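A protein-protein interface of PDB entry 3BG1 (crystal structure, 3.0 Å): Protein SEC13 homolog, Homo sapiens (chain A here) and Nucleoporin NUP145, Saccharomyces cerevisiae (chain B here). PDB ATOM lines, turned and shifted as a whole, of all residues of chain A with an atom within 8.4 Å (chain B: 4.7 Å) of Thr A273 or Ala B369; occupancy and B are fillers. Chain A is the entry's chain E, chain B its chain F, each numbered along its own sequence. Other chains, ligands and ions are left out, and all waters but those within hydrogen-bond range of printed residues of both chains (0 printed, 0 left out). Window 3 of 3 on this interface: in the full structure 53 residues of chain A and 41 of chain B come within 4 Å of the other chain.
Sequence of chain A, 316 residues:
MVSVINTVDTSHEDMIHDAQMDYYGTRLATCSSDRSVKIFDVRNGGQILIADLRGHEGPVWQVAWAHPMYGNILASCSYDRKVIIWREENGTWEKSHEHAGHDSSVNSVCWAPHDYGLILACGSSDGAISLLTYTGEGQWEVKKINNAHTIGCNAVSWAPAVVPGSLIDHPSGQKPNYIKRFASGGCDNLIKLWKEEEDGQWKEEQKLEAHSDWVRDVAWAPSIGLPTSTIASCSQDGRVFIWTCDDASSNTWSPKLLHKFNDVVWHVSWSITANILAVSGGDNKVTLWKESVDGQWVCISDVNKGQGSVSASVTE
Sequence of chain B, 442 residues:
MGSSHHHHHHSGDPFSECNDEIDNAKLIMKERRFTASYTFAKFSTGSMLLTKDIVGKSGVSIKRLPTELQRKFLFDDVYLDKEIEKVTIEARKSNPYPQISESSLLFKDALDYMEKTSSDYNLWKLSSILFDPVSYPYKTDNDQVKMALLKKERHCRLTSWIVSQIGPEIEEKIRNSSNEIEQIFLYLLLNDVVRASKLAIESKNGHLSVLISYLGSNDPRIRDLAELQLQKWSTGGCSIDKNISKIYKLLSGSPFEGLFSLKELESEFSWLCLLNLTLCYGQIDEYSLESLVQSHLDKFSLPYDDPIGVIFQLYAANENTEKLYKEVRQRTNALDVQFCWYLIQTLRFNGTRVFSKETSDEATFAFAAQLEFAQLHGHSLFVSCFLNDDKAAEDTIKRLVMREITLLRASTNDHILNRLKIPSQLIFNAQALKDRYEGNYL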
ATOM      1  N   PRO A 222     -27.603  -8.933 -10.105  1.00  0.00           N
ATOM      2  CA  PRO A 222     -27.436 -10.011 -11.089  1.00  0.00           C
ATOM      3  C   PRO A 222     -28.115 -11.263 -10.597  1.00  0.00           C
ATOM      4  O   PRO A 222     -28.062 -11.570  -9.412  1.00  0.00           O
ATOM      5  CB  PRO A 222     -25.931 -10.177 -11.161  1.00  0.00           C
ATOM      6  CG  PRO A 222     -25.551 -10.010  -9.726  1.00  0.00           C
ATOM      7  CD  PRO A 222     -26.386  -8.801  -9.285  1.00  0.00           C
ATOM      8  N   SER A 223     -28.755 -11.977 -11.510  1.00  0.00           N
ATOM      9  CA  SER A 223     -29.461 -13.184 -11.136  1.00  0.00           C
ATOM     10  C   SER A 223     -28.502 -14.338 -10.974  1.00  0.00           C
ATOM     11  O   SER A 223     -27.798 -14.710 -11.916  1.00  0.00           O
ATOM     12  CB  SER A 223     -30.516 -13.552 -12.187  1.00  0.00           C
ATOM     13  OG  SER A 223     -29.914 -14.077 -13.357  1.00  0.00           O
ATOM     14  N   ILE A 224     -28.462 -14.888  -9.765  1.00  0.00           N
ATOM     15  CA  ILE A 224     -27.624 -16.043  -9.496  1.00  0.00           C
ATOM     16  C   ILE A 224     -28.400 -17.205 -10.120  1.00  0.00           C
ATOM     17  O   ILE A 224     -28.756 -18.161  -9.437  1.00  0.00           O
ATOM     18  CB  ILE A 224     -27.430 -16.279  -7.952  1.00  0.00           C
ATOM     19  CG1 ILE A 224     -28.717 -15.959  -7.173  1.00  0.00           C
ATOM     20  CG2 ILE A 224     -26.250 -15.453  -7.448  1.00  0.00           C
ATOM     21  CD1 ILE A 224     -28.581 -16.157  -5.667  1.00  0.00           C
ATOM     22  N   GLY A 225     -28.676 -17.097 -11.422  1.00  0.00           N
ATOM     23  CA  GLY A 225     -29.438 -18.119 -12.130  1.00  0.00           C
ATOM     24  C   GLY A 225     -30.884 -18.129 -11.657  1.00  0.00           C
ATOM     25  O   GLY A 225     -31.799 -18.560 -12.375  1.00  0.00           O
ATOM     26  N   TRP A 270     -24.335  -4.155  -6.201  1.00  0.00           N
ATOM     27  CA  TRP A 270     -24.550  -5.542  -5.852  1.00  0.00           C
ATOM     28  C   TRP A 270     -23.309  -6.398  -5.904  1.00  0.00           C
ATOM     29  O   TRP A 270     -22.574  -6.386  -6.890  1.00  0.00           O
ATOM     30  CB  TRP A 270     -25.622  -6.166  -6.775  1.00  0.00           C
ATOM     31  CG  TRP A 270     -27.031  -5.697  -6.511  1.00  0.00           C
ATOM     32  CD1 TRP A 270     -27.759  -4.792  -7.245  1.00  0.00           C
ATOM     33  CD2 TRP A 270     -27.835  -6.040  -5.389  1.00  0.00           C
ATOM     34  NE1 TRP A 270     -28.960  -4.551  -6.636  1.00  0.00           N
ATOM     35  CE2 TRP A 270     -29.029  -5.304  -5.492  1.00  0.00           C
ATOM     36  CE3 TRP A 270     -27.661  -6.895  -4.304  1.00  0.00           C
ATOM     37  CZ2 TRP A 270     -30.045  -5.403  -4.543  1.00  0.00           C
ATOM     38  CZ3 TRP A 270     -28.664  -6.996  -3.366  1.00  0.00           C
ATOM     39  CH2 TRP A 270     -29.843  -6.254  -3.486  1.00  0.00           C
ATOM     40  N   SER A 271     -23.068  -7.139  -4.829  1.00  0.00           N
ATOM     41  CA  SER A 271     -21.961  -8.065  -4.817  1.00  0.00           C
ATOM     42  C   SER A 271     -22.571  -9.297  -5.541  1.00  0.00           C
ATOM     43  O   SER A 271     -23.746  -9.608  -5.388  1.00  0.00           O
ATOM     44  CB  SER A 271     -21.474  -8.254  -3.373  1.00  0.00           C
ATOM     45  OG  SER A 271     -21.917  -9.423  -2.772  1.00  0.00           O
ATOM     46  N   ILE A 272     -21.759  -9.918  -6.377  1.00  0.00           N
ATOM     47  CA  ILE A 272     -22.124 -10.968  -7.324  1.00  0.00           C
ATOM     48  C   ILE A 272     -22.738 -12.291  -6.974  1.00  0.00           C
ATOM     49  O   ILE A 272     -23.602 -12.782  -7.699  1.00  0.00           O
ATOM     50  CB  ILE A 272     -20.917 -11.314  -8.209  1.00  0.00           C
ATOM     51  CG1 ILE A 272     -20.446 -10.083  -8.949  1.00  0.00           C
ATOM     52  CG2 ILE A 272     -21.249 -12.359  -9.211  1.00  0.00           C
ATOM     53  CD1 ILE A 272     -19.082 -10.234  -9.581  1.00  0.00           C
ATOM     54  N   THR A 273     -22.245 -12.881  -5.902  1.00  0.00           N
ATOM     55  CA  THR A 273     -22.667 -14.198  -5.461  1.00  0.00           C
ATOM     56  C   THR A 273     -23.748 -14.169  -4.413  1.00  0.00           C
ATOM     57  O   THR A 273     -24.803 -14.792  -4.565  1.00  0.00           O
ATOM     58  CB  THR A 273     -21.497 -14.965  -4.830  1.00  0.00           C
ATOM     59  OG1 THR A 273     -20.454 -15.146  -5.790  1.00  0.00           O
ATOM     60  CG2 THR A 273     -21.961 -16.310  -4.337  1.00  0.00           C
ATOM     61  N   ALA A 274     -23.469 -13.444  -3.342  1.00  0.00           N
ATOM     62  CA  ALA A 274     -24.389 -13.400  -2.214  1.00  0.00           C
ATOM     63  C   ALA A 274     -25.521 -12.428  -2.407  1.00  0.00           C
ATOM     64  O   ALA A 274     -26.597 -12.577  -1.828  1.00  0.00           O
ATOM     65  CB  ALA A 274     -23.630 -13.050  -0.948  1.00  0.00           C
ATOM     66  N   ASN A 275     -25.272 -11.449  -3.250  1.00  0.00           N
ATOM     67  CA  ASN A 275     -26.248 -10.430  -3.505  1.00  0.00           C
ATOM     68  C   ASN A 275     -26.140  -9.469  -2.318  1.00  0.00           C
ATOM     69  O   ASN A 275     -27.128  -8.995  -1.768  1.00  0.00           O
ATOM     70  CB  ASN A 275     -27.641 -11.064  -3.696  1.00  0.00           C
ATOM     71  CG  ASN A 275     -27.648 -12.051  -4.871  1.00  0.00           C
ATOM     72  OD1 ASN A 275     -27.040 -11.785  -5.910  1.00  0.00           O
ATOM     73  ND2 ASN A 275     -28.326 -13.184  -4.712  1.00  0.00           N
ATOM     74  N   ILE A 276     -24.893  -9.191  -1.938  1.00  0.00           N
ATOM     75  CA  ILE A 276     -24.639  -8.242  -0.857  1.00  0.00           C
ATOM     76  C   ILE A 276     -24.681  -6.817  -1.368  1.00  0.00           C
ATOM     77  O   ILE A 276     -24.106  -6.469  -2.409  1.00  0.00           O
ATOM     78  CB  ILE A 276     -23.309  -8.492  -0.207  1.00  0.00           C
ATOM     79  CG1 ILE A 276     -23.330  -9.909   0.331  1.00  0.00           C
ATOM     80  CG2 ILE A 276     -23.069  -7.453   0.895  1.00  0.00           C
ATOM     81  CD1 ILE A 276     -22.123 -10.281   1.052  1.00  0.00           C
ATOM     82  N   LYS A 290     -26.852  -7.843   3.707  1.00  0.00           N
ATOM     83  CA  LYS A 290     -27.262  -9.154   3.259  1.00  0.00           C
ATOM     84  C   LYS A 290     -28.630  -9.423   3.878  1.00  0.00           C
ATOM     85  O   LYS A 290     -28.858  -9.145   5.058  1.00  0.00           O
ATOM     86  CB  LYS A 290     -26.264 -10.216   3.701  1.00  0.00           C
ATOM     87  CG  LYS A 290     -26.513 -11.534   3.018  1.00  0.00           C
ATOM     88  CD  LYS A 290     -25.385 -12.500   3.196  1.00  0.00           C
ATOM     89  CE  LYS A 290     -25.598 -13.652   2.250  1.00  0.00           C
ATOM     90  NZ  LYS A 290     -24.507 -14.632   2.345  1.00  0.00           N
ATOM     91  N   PHE B 365     -25.341 -22.671  -2.800  1.00  0.00           N
ATOM     92  CA  PHE B 365     -24.854 -21.372  -3.238  1.00  0.00           C
ATOM     93  C   PHE B 365     -24.049 -20.813  -2.099  1.00  0.00           C
ATOM     94  O   PHE B 365     -22.878 -20.477  -2.259  1.00  0.00           O
ATOM     95  CB  PHE B 365     -26.001 -20.403  -3.524  1.00  0.00           C
ATOM     96  CG  PHE B 365     -26.670 -20.629  -4.840  1.00  0.00           C
ATOM     97  CD1 PHE B 365     -27.825 -19.934  -5.168  1.00  0.00           C
ATOM     98  CD2 PHE B 365     -26.156 -21.554  -5.747  1.00  0.00           C
ATOM     99  CE1 PHE B 365     -28.459 -20.159  -6.375  1.00  0.00           C
ATOM    100  CE2 PHE B 365     -26.783 -21.786  -6.958  1.00  0.00           C
ATOM    101  CZ  PHE B 365     -27.935 -21.090  -7.273  1.00  0.00           C
ATOM    102  N   ALA B 366     -24.698 -20.728  -0.943  1.00  0.00           N
ATOM    103  CA  ALA B 366     -24.079 -20.193   0.255  1.00  0.00           C
ATOM    104  C   ALA B 366     -22.593 -20.529   0.335  1.00  0.00           C
ATOM    105  O   ALA B 366     -21.743 -19.635   0.318  1.00  0.00           O
ATOM    106  CB  ALA B 366     -24.803 -20.724   1.472  1.00  0.00           C
ATOM    107  N   PHE B 367     -22.297 -21.824   0.413  1.00  0.00           N
ATOM    108  CA  PHE B 367     -20.926 -22.339   0.514  1.00  0.00           C
ATOM    109  C   PHE B 367     -20.078 -21.974  -0.706  1.00  0.00           C
ATOM    110  O   PHE B 367     -19.056 -21.311  -0.581  1.00  0.00           O
ATOM    111  CB  PHE B 367     -20.998 -23.857   0.687  1.00  0.00           C
ATOM    112  CG  PHE B 367     -19.685 -24.525   0.975  1.00  0.00           C
ATOM    113  CD1 PHE B 367     -18.873 -24.089   2.012  1.00  0.00           C
ATOM    114  CD2 PHE B 367     -19.315 -25.673   0.274  1.00  0.00           C
ATOM    115  CE1 PHE B 367     -17.712 -24.794   2.352  1.00  0.00           C
ATOM    116  CE2 PHE B 367     -18.157 -26.388   0.608  1.00  0.00           C
ATOM    117  CZ  PHE B 367     -17.356 -25.948   1.651  1.00  0.00           C
ATOM    118  N   ALA B 368     -20.518 -22.398  -1.884  1.00  0.00           N
ATOM    119  CA  ALA B 368     -19.805 -22.129  -3.131  1.00  0.00           C
ATOM    120  C   ALA B 368     -19.461 -20.658  -3.298  1.00  0.00           C
ATOM    121  O   ALA B 368     -18.654 -20.293  -4.150  1.00  0.00           O
ATOM    122  CB  ALA B 368     -20.637 -22.598  -4.316  1.00  0.00           C
ATOM    123  N   ALA B 369     -20.083 -19.816  -2.483  1.00  0.00           N
ATOM    124  CA  ALA B 369     -19.855 -18.378  -2.526  1.00  0.00           C
ATOM    125  C   ALA B 369     -18.650 -18.010  -1.677  1.00  0.00           C
ATOM    126  O   ALA B 369     -17.761 -17.265  -2.101  1.00  0.00           O
ATOM    127  CB  ALA B 369     -21.061 -17.677  -1.999  1.00  0.00           C
ATOM    128  N   GLN B 370     -18.649 -18.518  -0.452  1.00  0.00           N
ATOM    129  CA  GLN B 370     -17.555 -18.269   0.460  1.00  0.00           C
ATOM    130  C   GLN B 370     -16.294 -18.732  -0.239  1.00  0.00           C
ATOM    131  O   GLN B 370     -15.269 -18.065  -0.213  1.00  0.00           O
ATOM    132  CB  GLN B 370     -17.777 -19.042   1.756  1.00  0.00           C
ATOM    133  CG  GLN B 370     -18.990 -18.551   2.508  1.00  0.00           C
ATOM    134  CD  GLN B 370     -18.898 -17.064   2.822  1.00  0.00           C
ATOM    135  OE1 GLN B 370     -18.373 -16.280   2.025  1.00  0.00           O
ATOM    136  NE2 GLN B 370     -19.426 -16.666   3.980  1.00  0.00           N
ATOM    137  N   LEU B 371     -16.387 -19.878  -0.891  1.00  0.00           N
ATOM    138  CA  LEU B 371     -15.252 -20.401  -1.608  1.00  0.00           C
ATOM    139  C   LEU B 371     -14.841 -19.472  -2.745  1.00  0.00           C
ATOM    140  O   LEU B 371     -13.726 -19.565  -3.255  1.00  0.00           O
ATOM    141  CB  LEU B 371     -15.577 -21.782  -2.170  1.00  0.00           C
ATOM    142  CG  LEU B 371     -16.047 -22.783  -1.116  1.00  0.00           C
ATOM    143  CD1 LEU B 371     -16.185 -24.154  -1.750  1.00  0.00           C
ATOM    144  CD2 LEU B 371     -15.059 -22.827   0.033  1.00  0.00           C
ATOM    145  N   GLU B 372     -15.731 -18.583  -3.159  1.00  0.00           N
ATOM    146  CA  GLU B 372     -15.382 -17.696  -4.251  1.00  0.00           C
ATOM    147  C   GLU B 372     -14.655 -16.454  -3.723  1.00  0.00           C
ATOM    148  O   GLU B 372     -13.705 -15.963  -4.352  1.00  0.00           O
ATOM    149  CB  GLU B 372     -16.626 -17.263  -5.019  1.00  0.00           C
ATOM    150  CG  GLU B 372     -16.327 -16.904  -6.457  1.00  0.00           C
ATOM    151  CD  GLU B 372     -17.577 -16.629  -7.255  1.00  0.00           C
ATOM    152  OE1 GLU B 372     -18.515 -17.459  -7.202  1.00  0.00           O
ATOM    153  OE2 GLU B 372     -17.619 -15.588  -7.941  1.00  0.00           O
ATOM    154  N   PHE B 373     -15.108 -15.955  -2.559  1.00  0.00           N
ATOM    155  CA  PHE B 373     -14.434 -14.819  -1.936  1.00  0.00           C
ATOM    156  C   PHE B 373     -13.034 -15.239  -1.557  1.00  0.00           C
ATOM    157  O   PHE B 373     -12.096 -14.429  -1.612  1.00  0.00           O
ATOM    158  CB  PHE B 373     -15.167 -14.364  -0.707  1.00  0.00           C
ATOM    159  CG  PHE B 373     -16.550 -14.007  -1.035  1.00  0.00           C
ATOM    160  CD1 PHE B 373     -17.578 -14.879  -0.707  1.00  0.00           C
ATOM    161  CD2 PHE B 373     -16.834 -12.801  -1.640  1.00  0.00           C
ATOM    162  CE1 PHE B 373     -18.877 -14.550  -0.979  1.00  0.00           C
ATOM    163  CE2 PHE B 373     -18.127 -12.456  -1.921  1.00  0.00           C
ATOM    164  CZ  PHE B 373     -19.160 -13.330  -1.589  1.00  0.00           C
ATOM    165  N   ARG B 399     -19.897 -18.652 -15.803  1.00  0.00           N
ATOM    166  CA  ARG B 399     -19.369 -17.422 -15.211  1.00  0.00           C
ATOM    167  C   ARG B 399     -18.032 -17.603 -14.513  1.00  0.00           C
ATOM    168  O   ARG B 399     -17.036 -16.971 -14.876  1.00  0.00           O
ATOM    169  CB  ARG B 399     -20.355 -16.843 -14.203  1.00  0.00           C
ATOM    170  CG  ARG B 399     -19.940 -15.480 -13.692  1.00  0.00           C
ATOM    171  CD  ARG B 399     -20.865 -15.039 -12.588  1.00  0.00           C
ATOM    172  NE  ARG B 399     -20.655 -15.846 -11.395  1.00  0.00           N
ATOM    173  CZ  ARG B 399     -19.665 -15.649 -10.527  1.00  0.00           C
ATOM    174  NH1 ARG B 399     -18.799 -14.662 -10.725  1.00  0.00           N
ATOM    175  NH2 ARG B 399     -19.537 -16.449  -9.471  1.00  0.00           N
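The side-chain hydroxyl of Thr A273 lies within hydrogen-bond range of the side-chain carboxylate of Glu B372, at 3.3 Å.
The side-chain carboxylate of Glu B372 lies within salt-bridge range of the guanidinium group of Arg B399 (2.6 Å).
Among the printed residues, merely in contact across the chains: Thr A273 with Ala B369, Ile A224 with Phe B365 and Ile A272 with Arg B399.
Printed residues of chain B within 4 Å of Ile A224: Phe B365 (3.7 Å). Of the printed residues of chain B, Ile A272 touches Arg B399 (3.7 Å). Of the printed residues of chain B, Thr A273 touches Ala B369 and Glu B372. Printed residues of chain A within 4 Å of Phe B365: Ile A224. Ala B368 touches none of the printed residues of chain A. Of chain A, only Thr A273 (2.9 Å) comes within 4 Å of Ala B369. Printed residues of chain A within 4 Å of Glu B372: Thr A273 (3.3 Å). Of the printed residues of chain A, Arg B399 touches Ile A272 (3.7 Å). The nearest printed residue of chain B that does not touch Thr A273 is Arg B399 (4.01 Å).
Of the 10 printed residues of chain B, 4 touch a printed residue of chain A. Hydrophobic or aromatic side chains of chain A within 4 Å of the printed part of chain B: Ile A224 and Ile A272. Among the printed residues, no Asp or Glu carboxylate lies within 4 Å of a Lys or Arg side-chain nitrogen of the other chain.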
